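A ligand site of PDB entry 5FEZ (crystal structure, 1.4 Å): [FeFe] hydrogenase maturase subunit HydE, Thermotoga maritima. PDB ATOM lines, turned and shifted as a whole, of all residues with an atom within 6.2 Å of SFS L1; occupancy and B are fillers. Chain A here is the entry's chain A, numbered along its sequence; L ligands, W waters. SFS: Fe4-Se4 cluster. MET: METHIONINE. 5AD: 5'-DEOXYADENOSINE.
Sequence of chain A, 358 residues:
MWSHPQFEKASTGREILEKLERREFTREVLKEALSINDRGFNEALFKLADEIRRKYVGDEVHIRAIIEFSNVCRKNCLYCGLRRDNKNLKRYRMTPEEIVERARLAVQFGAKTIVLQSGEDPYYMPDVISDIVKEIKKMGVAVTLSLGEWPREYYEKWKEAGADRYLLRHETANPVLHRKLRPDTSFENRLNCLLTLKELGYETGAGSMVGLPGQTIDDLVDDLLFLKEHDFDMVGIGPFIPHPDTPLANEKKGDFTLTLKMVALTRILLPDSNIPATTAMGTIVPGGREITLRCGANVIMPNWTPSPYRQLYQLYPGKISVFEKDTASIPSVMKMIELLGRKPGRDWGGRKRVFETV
The backbone NH of Leu 82 sits close to the side-chain sulfur of Cys 80, at 3.4 Å.
The side-chain sulfur (SG) of Cys 73 lies close to the backbone NH (N) of Lys 75 (3.3 Å).
SG of Cys 73 lies close to N of Glu 120 (3.3 Å).
The backbone carbonyl oxygen of Cys 77 is in hydrogen-bond range of the guanidinium group of Arg 83.
SG of Cys 77 lies close to NE of Arg 182, 3.6 Å away.
The guanidinium group (NH2) of Arg 83 lies within hydrogen-bond range of the backbone carbonyl oxygen (O) of Asn 76 (2.9 Å).
NZ of Lys 75 lies within salt-bridge range of OE1 of Glu 120 (2.7 Å).
The backbone carbonyl oxygen (O) of Lys 75 is in hydrogen-bond range of the backbone NH (N) of Arg 84 (2.9 Å).
An iron atom (FE4) of SFS L1 is bound by a nitrogen (N) of MET L2, 2.2 Å away.
SG of Cys 80 binds FE1 of SFS L1, at 2.3 Å.
The side-chain sulfur (SG) of Cys 73 binds an iron atom (FE2) of SFS L1 (2.3 Å).
SG of Cys 77 binds FE3 of SFS L1 (2.3 Å).
A nitrogen (N) of MET L2 sits close to the backbone carbonyl oxygen (O) of Ser 118, at 3.3 Å.
An oxygen (O) of MET L2 is in salt-bridge range of the guanidinium group (NH2) of Arg 190.
The backbone carbonyl oxygen of Tyr 79 lies within hydrogen-bond range of a nitrogen (N6) of 5AD L3 (2.9 Å).
The side-chain carboxylate of Glu 171 is in hydrogen-bond range of an oxygen (O3') of 5AD L3.
Water W1 lies within hydrogen-bond range of the side-chain carboxylate (OE2) of Glu 171 (2.7 Å), the side-chain hydroxyl (OH) of Tyr 79 (2.7 Å) and the guanidinium group (NE) of Arg 182 (3.1 Å).
Water W2 lies within hydrogen-bond range of the side-chain carboxylate of Glu 120 (2.7 Å), the guanidinium group of Arg 190 (2.8 Å), the guanidinium group of Arg 182 (3.3 Å) and an oxygen (O) of MET L2 (3.4 Å).
CD of Lys 75 touches SE1 of SFS L1 (3.8 Å).
CE1 of Tyr 79 touches SE2 of SFS L1, 3.7 Å away.
Arg 83 touches SFS L1 (CA to SE4, 3.7 Å).
Gly 119 touches SFS L1 (CA to SE3, 3.7 Å).
Within 4 Å of SFS L1: Cys 73, Lys 75, Cys 77, Tyr 79, Cys 80, Arg 83 and Gly 119.
The nearest printed residue that does not touch SFS L1 is Leu 82 (4.03 Å).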
ATOM      1  N   VAL A  72       1.930   5.049  -4.551  1.00  0.00           N
ATOM      2  CA  VAL A  72       2.908   3.957  -4.720  1.00  0.00           C
ATOM      3  C   VAL A  72       2.190   2.650  -4.386  1.00  0.00           C
ATOM      4  O   VAL A  72       1.535   2.531  -3.355  1.00  0.00           O
ATOM      5  CB  VAL A  72       4.101   4.146  -3.808  1.00  0.00           C
ATOM      6  CG1 VAL A  72       5.022   2.892  -3.837  1.00  0.00           C
ATOM      7  CG2 VAL A  72       4.859   5.409  -4.227  1.00  0.00           C
ATOM      8  N   CYS A  73       2.341   1.659  -5.268  1.00  0.00           N
ATOM      9  CA  CYS A  73       1.799   0.331  -4.957  1.00  0.00           C
ATOM     10  C   CYS A  73       2.700  -0.809  -5.368  1.00  0.00           C
ATOM     11  O   CYS A  73       3.325  -0.766  -6.399  1.00  0.00           O
ATOM     12  CB  CYS A  73       0.439   0.079  -5.656  1.00  0.00           C
ATOM     13  SG  CYS A  73      -0.410  -1.345  -4.852  1.00  0.00           S
ATOM     14  N   ARG A  74       2.785  -1.792  -4.512  1.00  0.00           N
ATOM     15  CA  ARG A  74       3.570  -3.011  -4.787  1.00  0.00           C
ATOM     16  C   ARG A  74       2.763  -4.059  -5.564  1.00  0.00           C
ATOM     17  O   ARG A  74       3.402  -5.023  -6.081  1.00  0.00           O
ATOM     18  CB  ARG A  74       4.031  -3.639  -3.472  1.00  0.00           C
ATOM     19  CG  ARG A  74       2.887  -4.226  -2.637  1.00  0.00           C
ATOM     20  CD  ARG A  74       3.325  -4.685  -1.316  1.00  0.00           C
ATOM     21  NE  ARG A  74       2.237  -5.130  -0.489  1.00  0.00           N
ATOM     22  CZ  ARG A  74       2.352  -5.860   0.592  1.00  0.00           C
ATOM     23  NH1 ARG A  74       3.515  -6.268   1.024  1.00  0.00           N
ATOM     24  NH2 ARG A  74       1.273  -6.235   1.253  1.00  0.00           N
ATOM     25  N   LYS A  75       1.455  -3.947  -5.680  1.00  0.00           N
ATOM     26  CA  LYS A  75       0.615  -4.921  -6.373  1.00  0.00           C
ATOM     27  C   LYS A  75       0.373  -4.493  -7.815  1.00  0.00           C
ATOM     28  O   LYS A  75       0.728  -3.397  -8.237  1.00  0.00           O
ATOM     29  CB  LYS A  75      -0.678  -5.160  -5.612  1.00  0.00           C
ATOM     30  CG  LYS A  75      -0.521  -6.106  -4.394  1.00  0.00           C
ATOM     31  CD  LYS A  75      -1.845  -6.440  -3.775  1.00  0.00           C
ATOM     32  CE  LYS A  75      -1.798  -7.601  -2.779  1.00  0.00           C
ATOM     33  NZ  LYS A  75      -0.738  -7.487  -1.745  1.00  0.00           N
ATOM     34  N   ASN A  76      -0.268  -5.392  -8.583  1.00  0.00           N
ATOM     35  CA  ASN A  76      -0.378  -5.260 -10.018  1.00  0.00           C
ATOM     36  C   ASN A  76      -1.773  -5.583 -10.506  1.00  0.00           C
ATOM     37  O   ASN A  76      -1.946  -6.155 -11.590  1.00  0.00           O
ATOM     38  CB  ASN A  76       0.632  -6.153 -10.697  1.00  0.00           C
ATOM     39  CG  ASN A  76       1.146  -5.599 -12.009  1.00  0.00           C
ATOM     40  OD1 ASN A  76       1.172  -4.420 -12.282  1.00  0.00           O
ATOM     41  ND2 ASN A  76       1.695  -6.524 -12.868  1.00  0.00           N
ATOM     42  N   CYS A  77      -2.791  -5.276  -9.715  1.00  0.00           N
ATOM     43  CA  CYS A  77      -4.173  -5.588 -10.132  1.00  0.00           C
ATOM     44  C   CYS A  77      -4.460  -5.086 -11.540  1.00  0.00           C
ATOM     45  O   CYS A  77      -4.095  -4.021 -11.923  1.00  0.00           O
ATOM     46  CB  CYS A  77      -5.135  -4.942  -9.133  1.00  0.00           C
ATOM     47  SG  CYS A  77      -4.808  -5.329  -7.377  1.00  0.00           S
ATOM     48  N   TYR A  79      -7.017  -4.121 -13.171  1.00  0.00           N
ATOM     49  CA  TYR A  79      -7.979  -3.026 -13.392  1.00  0.00           C
ATOM     50  C   TYR A  79      -7.476  -1.638 -13.026  1.00  0.00           C
ATOM     51  O   TYR A  79      -8.094  -0.642 -13.425  1.00  0.00           O
ATOM     52  CB  TYR A  79      -9.301  -3.303 -12.674  1.00  0.00           C
ATOM     53  CG  TYR A  79      -9.171  -3.810 -11.262  1.00  0.00           C
ATOM     54  CD1 TYR A  79      -8.924  -2.909 -10.221  1.00  0.00           C
ATOM     55  CD2 TYR A  79      -9.214  -5.156 -10.933  1.00  0.00           C
ATOM     56  CE1 TYR A  79      -8.755  -3.351  -8.934  1.00  0.00           C
ATOM     57  CE2 TYR A  79      -9.018  -5.573  -9.646  1.00  0.00           C
ATOM     58  CZ  TYR A  79      -8.802  -4.656  -8.635  1.00  0.00           C
ATOM     59  OH  TYR A  79      -8.630  -5.151  -7.361  1.00  0.00           O
ATOM     60  N   CYS A  80      -6.410  -1.593 -12.238  1.00  0.00           N
ATOM     61  CA  CYS A  80      -6.085  -0.388 -11.493  1.00  0.00           C
ATOM     62  C   CYS A  80      -5.016   0.497 -12.087  1.00  0.00           C
ATOM     63  O   CYS A  80      -3.918   0.008 -12.374  1.00  0.00           O
ATOM     64  CB  CYS A  80      -5.647  -0.770 -10.093  1.00  0.00           C
ATOM     65  SG  CYS A  80      -5.306   0.618  -8.965  1.00  0.00           S
ATOM     66  N   GLY A  81      -5.267   1.796 -12.243  1.00  0.00           N
ATOM     67  CA  GLY A  81      -4.277   2.683 -12.736  1.00  0.00           C
ATOM     68  C   GLY A  81      -3.026   2.886 -11.904  1.00  0.00           C
ATOM     69  O   GLY A  81      -2.040   3.434 -12.419  1.00  0.00           O
ATOM     70  N   LEU A  82      -3.025   2.469 -10.651  1.00  0.00           N
ATOM     71  CA  LEU A  82      -1.871   2.530  -9.803  1.00  0.00           C
ATOM     72  C   LEU A  82      -1.014   1.259  -9.815  1.00  0.00           C
ATOM     73  O   LEU A  82       0.007   1.215  -9.153  1.00  0.00           O
ATOM     74  CB  LEU A  82      -2.226   2.873  -8.340  1.00  0.00           C
ATOM     75  CG  LEU A  82      -3.030   4.123  -8.123  1.00  0.00           C
ATOM     76  CD1 LEU A  82      -3.142   4.423  -6.649  1.00  0.00           C
ATOM     77  CD2 LEU A  82      -2.734   5.302  -8.920  1.00  0.00           C
ATOM     78  N   ARG A  83      -1.394   0.290 -10.614  1.00  0.00           N
ATOM     79  CA  ARG A  83      -0.657  -0.984 -10.618  1.00  0.00           C
ATOM     80  C   ARG A  83       0.803  -0.740 -10.862  1.00  0.00           C
ATOM     81  O   ARG A  83       1.223   0.147 -11.594  1.00  0.00           O
ATOM     82  CB  ARG A  83      -1.260  -1.920 -11.678  1.00  0.00           C
ATOM     83  CG  ARG A  83      -1.119  -1.444 -13.123  1.00  0.00           C
ATOM     84  CD  ARG A  83      -2.057  -2.183 -14.038  1.00  0.00           C
ATOM     85  NE  ARG A  83      -1.971  -3.631 -13.890  1.00  0.00           N
ATOM     86  CZ  ARG A  83      -1.170  -4.437 -14.583  1.00  0.00           C
ATOM     87  NH1 ARG A  83      -0.403  -3.916 -15.516  1.00  0.00           N
ATOM     88  NH2 ARG A  83      -1.171  -5.695 -14.335  1.00  0.00           N
ATOM     89  N   ARG A  84       1.641  -1.610 -10.270  1.00  0.00           N
ATOM     90  CA  ARG A  84       3.096  -1.364 -10.326  1.00  0.00           C
ATOM     91  C   ARG A  84       3.660  -1.330 -11.735  1.00  0.00           C
ATOM     92  O   ARG A  84       4.644  -0.619 -11.947  1.00  0.00           O
ATOM     93  CB  ARG A  84       3.868  -2.327  -9.480  1.00  0.00           C
ATOM     94  CG  ARG A  84       3.871  -3.753  -9.951  1.00  0.00           C
ATOM     95  CD  ARG A  84       4.863  -4.623  -9.143  1.00  0.00           C
ATOM     96  NE  ARG A  84       4.827  -5.926  -9.768  1.00  0.00           N
ATOM     97  CZ  ARG A  84       4.062  -6.933  -9.380  1.00  0.00           C
ATOM     98  NH1 ARG A  84       3.317  -6.884  -8.293  1.00  0.00           N
ATOM     99  NH2 ARG A  84       3.976  -7.977 -10.159  1.00  0.00           N
ATOM    100  N   SER A 118      -4.353   4.619   0.364  1.00  0.00           N
ATOM    101  CA  SER A 118      -3.142   4.627  -0.446  1.00  0.00           C
ATOM    102  C   SER A 118      -3.068   3.379  -1.282  1.00  0.00           C
ATOM    103  O   SER A 118      -3.773   2.381  -1.040  1.00  0.00           O
ATOM    104  CB  SER A 118      -1.893   4.751   0.450  1.00  0.00           C
ATOM    105  OG  SER A 118      -1.770   3.658   1.328  1.00  0.00           O
ATOM    106  N   GLY A 119      -2.138   3.391  -2.219  1.00  0.00           N
ATOM    107  CA  GLY A 119      -1.603   2.140  -2.756  1.00  0.00           C
ATOM    108  C   GLY A 119      -1.007   1.316  -1.629  1.00  0.00           C
ATOM    109  O   GLY A 119      -0.752   1.830  -0.507  1.00  0.00           O
ATOM    110  N   GLU A 120      -0.703   0.064  -1.855  1.00  0.00           N
ATOM    111  CA  GLU A 120       0.026  -0.740  -0.918  1.00  0.00           C
ATOM    112  C   GLU A 120       1.498  -0.311  -0.941  1.00  0.00           C
ATOM    113  O   GLU A 120       2.353  -0.935  -1.640  1.00  0.00           O
ATOM    114  CB  GLU A 120      -0.112  -2.233  -1.165  1.00  0.00           C
ATOM    115  CG  GLU A 120      -1.511  -2.755  -0.882  1.00  0.00           C
ATOM    116  CD  GLU A 120      -1.591  -4.261  -0.794  1.00  0.00           C
ATOM    117  OE1 GLU A 120      -0.532  -4.924  -0.873  1.00  0.00           O
ATOM    118  OE2 GLU A 120      -2.721  -4.802  -0.675  1.00  0.00           O
ATOM    119  N   GLY A 148      -5.076  -1.646   2.044  1.00  0.00           N
ATOM    120  CA  GLY A 148      -4.826  -2.942   1.402  1.00  0.00           C
ATOM    121  C   GLY A 148      -4.580  -4.076   2.399  1.00  0.00           C
ATOM    122  O   GLY A 148      -4.966  -4.021   3.557  1.00  0.00           O
ATOM    123  N   GLU A 171     -13.826  -6.979  -3.868  1.00  0.00           N
ATOM    124  CA  GLU A 171     -13.641  -6.821  -5.312  1.00  0.00           C
ATOM    125  C   GLU A 171     -14.529  -7.702  -6.189  1.00  0.00           C
ATOM    126  O   GLU A 171     -15.275  -7.235  -7.000  1.00  0.00           O
ATOM    127  CB  GLU A 171     -12.157  -6.920  -5.711  1.00  0.00           C
ATOM    128  CG  GLU A 171     -11.182  -6.091  -4.864  1.00  0.00           C
ATOM    129  CD  GLU A 171     -11.401  -4.610  -4.951  1.00  0.00           C
ATOM    130  OE1 GLU A 171     -12.352  -4.103  -5.517  1.00  0.00           O
ATOM    131  OE2 GLU A 171     -10.565  -3.909  -4.365  1.00  0.00           O
ATOM    132  N   ARG A 182      -6.214 -10.119  -9.761  1.00  0.00           N
ATOM    133  CA  ARG A 182      -5.340  -9.713  -8.655  1.00  0.00           C
ATOM    134  C   ARG A 182      -4.268 -10.812  -8.439  1.00  0.00           C
ATOM    135  O   ARG A 182      -4.259 -11.559  -7.531  1.00  0.00           O
ATOM    136  CB  ARG A 182      -6.188  -9.467  -7.405  1.00  0.00           C
ATOM    137  CG  ARG A 182      -7.393  -8.566  -7.657  1.00  0.00           C
ATOM    138  CD  ARG A 182      -8.142  -8.128  -6.422  1.00  0.00           C
ATOM    139  NE  ARG A 182      -7.257  -7.261  -5.621  1.00  0.00           N
ATOM    140  CZ  ARG A 182      -6.713  -7.550  -4.483  1.00  0.00           C
ATOM    141  NH1 ARG A 182      -7.048  -8.583  -3.804  1.00  0.00           N
ATOM    142  NH2 ARG A 182      -5.804  -6.687  -3.999  1.00  0.00           N
ATOM    143  N   ARG A 190      -7.914 -12.195   0.787  1.00  0.00           N
ATOM    144  CA  ARG A 190      -8.774 -11.015   0.994  1.00  0.00           C
ATOM    145  C   ARG A 190      -9.770 -11.228   2.096  1.00  0.00           C
ATOM    146  O   ARG A 190      -9.967 -10.400   2.992  1.00  0.00           O
ATOM    147  CB  ARG A 190      -9.475 -10.692  -0.335  1.00  0.00           C
ATOM    148  CG  ARG A 190     -10.062  -9.265  -0.458  1.00  0.00           C
ATOM    149  CD  ARG A 190      -8.930  -8.300  -0.682  1.00  0.00           C
ATOM    150  NE  ARG A 190      -9.411  -6.954  -1.074  1.00  0.00           N
ATOM    151  CZ  ARG A 190      -8.594  -5.905  -1.244  1.00  0.00           C
ATOM    152  NH1 ARG A 190      -7.292  -6.065  -1.116  1.00  0.00           N
ATOM    153  NH2 ARG A 190      -9.122  -4.746  -1.512  1.00  0.00           N
ATOM    154  N   TYR A 313      -3.708  10.490  -8.553  1.00  0.00           N
ATOM    155  CA  TYR A 313      -4.351   9.317  -7.929  1.00  0.00           C
ATOM    156  C   TYR A 313      -5.580   8.968  -8.733  1.00  0.00           C
ATOM    157  O   TYR A 313      -6.685   9.318  -8.383  1.00  0.00           O
ATOM    158  CB  TYR A 313      -4.692   9.573  -6.488  1.00  0.00           C
ATOM    159  CG  TYR A 313      -4.952   8.319  -5.621  1.00  0.00           C
ATOM    160  CD1 TYR A 313      -3.978   7.758  -4.849  1.00  0.00           C
ATOM    161  CD2 TYR A 313      -6.193   7.739  -5.552  1.00  0.00           C
ATOM    162  CE1 TYR A 313      -4.211   6.700  -4.030  1.00  0.00           C
ATOM    163  CE2 TYR A 313      -6.438   6.695  -4.718  1.00  0.00           C
ATOM    164  CZ  TYR A 313      -5.487   6.210  -3.965  1.00  0.00           C
ATOM    165  OH  TYR A 313      -5.649   5.204  -3.045  1.00  0.00           O
ATOM    166  N   LEU A 315      -7.291   5.835 -10.151  1.00  0.00           N
ATOM    167  CA  LEU A 315      -7.494   4.418 -10.236  1.00  0.00           C
ATOM    168  C   LEU A 315      -8.155   4.114 -11.575  1.00  0.00           C
ATOM    169  O   LEU A 315      -7.904   3.118 -12.184  1.00  0.00           O
ATOM    170  CB  LEU A 315      -8.428   3.957  -9.106  1.00  0.00           C
ATOM    171  CG  LEU A 315      -8.010   4.400  -7.709  1.00  0.00           C
ATOM    172  CD1 LEU A 315      -8.961   3.855  -6.673  1.00  0.00           C
ATOM    173  CD2 LEU A 315      -6.649   4.060  -7.450  1.00  0.00           C
HETATM  174 SE4  SFS L   1      -2.863  -2.108  -7.854  1.00  0.00          SE
HETATM  175 FE1  SFS L   1      -4.605  -0.558  -7.165  1.00  0.00          FE
HETATM  176 FE3  SFS L   1      -4.504  -3.187  -6.478  1.00  0.00          FE
HETATM  177 FE2  SFS L   1      -2.569  -1.453  -5.628  1.00  0.00          FE
HETATM  178 SE3  SFS L   1      -3.739   0.567  -5.404  1.00  0.00          SE
HETATM  179 FE4  SFS L   1      -5.231  -1.100  -4.391  1.00  0.00          FE
HETATM  180 SE2  SFS L   1      -6.470  -1.820  -6.430  1.00  0.00          SE
HETATM  181 SE1  SFS L   1      -3.622  -3.117  -4.294  1.00  0.00          SE
HETATM  182  N   MET L   2      -4.808  -0.531  -2.258  1.00  0.00           N
HETATM  183  CA  MET L   2      -5.947  -0.619  -1.318  1.00  0.00           C
HETATM  184  C   MET L   2      -6.888  -1.739  -1.753  1.00  0.00           C
HETATM  185  O   MET L   2      -7.719  -2.195  -0.997  1.00  0.00           O
HETATM  186  CB  MET L   2      -6.642   0.729  -1.287  1.00  0.00           C
HETATM  187  CG  MET L   2      -7.674   0.912  -2.398  1.00  0.00           C
HETATM  188  SD  MET L   2      -6.981   0.831  -4.055  1.00  0.00           S
HETATM  189  CE  MET L   2      -6.106   2.440  -3.911  1.00  0.00           C
HETATM  190  OXT MET L   2      -6.638  -2.125  -2.952  1.00  0.00           O
HETATM  191  N1  5AD L   3     -12.584   1.146 -12.023  1.00  0.00           N
HETATM  192  C2  5AD L   3     -13.390   1.309 -10.958  1.00  0.00           C
HETATM  193  N3  5AD L   3     -13.025   1.090  -9.684  1.00  0.00           N
HETATM  194  C4  5AD L   3     -11.778   0.763  -9.461  1.00  0.00           C
HETATM  195  N9  5AD L   3     -11.118   0.539  -8.350  1.00  0.00           N
HETATM  196  C8  5AD L   3      -9.845   0.284  -8.706  1.00  0.00           C
HETATM  197  N7  5AD L   3      -9.676   0.363  -9.993  1.00  0.00           N
HETATM  198  C5  5AD L   3     -10.876   0.681 -10.532  1.00  0.00           C
HETATM  199  C6  5AD L   3     -11.336   0.877 -11.853  1.00  0.00           C
HETATM  200  N6  5AD L   3     -10.523   0.783 -12.940  1.00  0.00           N
HETATM  201  C1' 5AD L   3     -11.750   0.380  -7.047  1.00  0.00           C
HETATM  202  C2' 5AD L   3     -11.456  -0.970  -6.397  1.00  0.00           C
HETATM  203  C3' 5AD L   3     -10.748  -0.568  -5.131  1.00  0.00           C
HETATM  204  C4' 5AD L   3     -11.334   0.791  -4.841  1.00  0.00           C
HETATM  205  C5' 5AD L   3     -10.388   1.673  -4.088  1.00  0.00           C
HETATM  206  O4' 5AD L   3     -11.309   1.373  -6.154  1.00  0.00           O
HETATM  207  O2' 5AD L   3     -12.719  -1.606  -6.146  1.00  0.00           O
HETATM  208  O3' 5AD L   3     -10.997  -1.418  -3.991  1.00  0.00           O
HETATM  209  O   HOH W   1      -7.912  -4.297  -4.856  1.00  0.00           O
HETATM  210  O   HOH W   2      -5.163  -4.379  -1.678  1.00  0.00           O
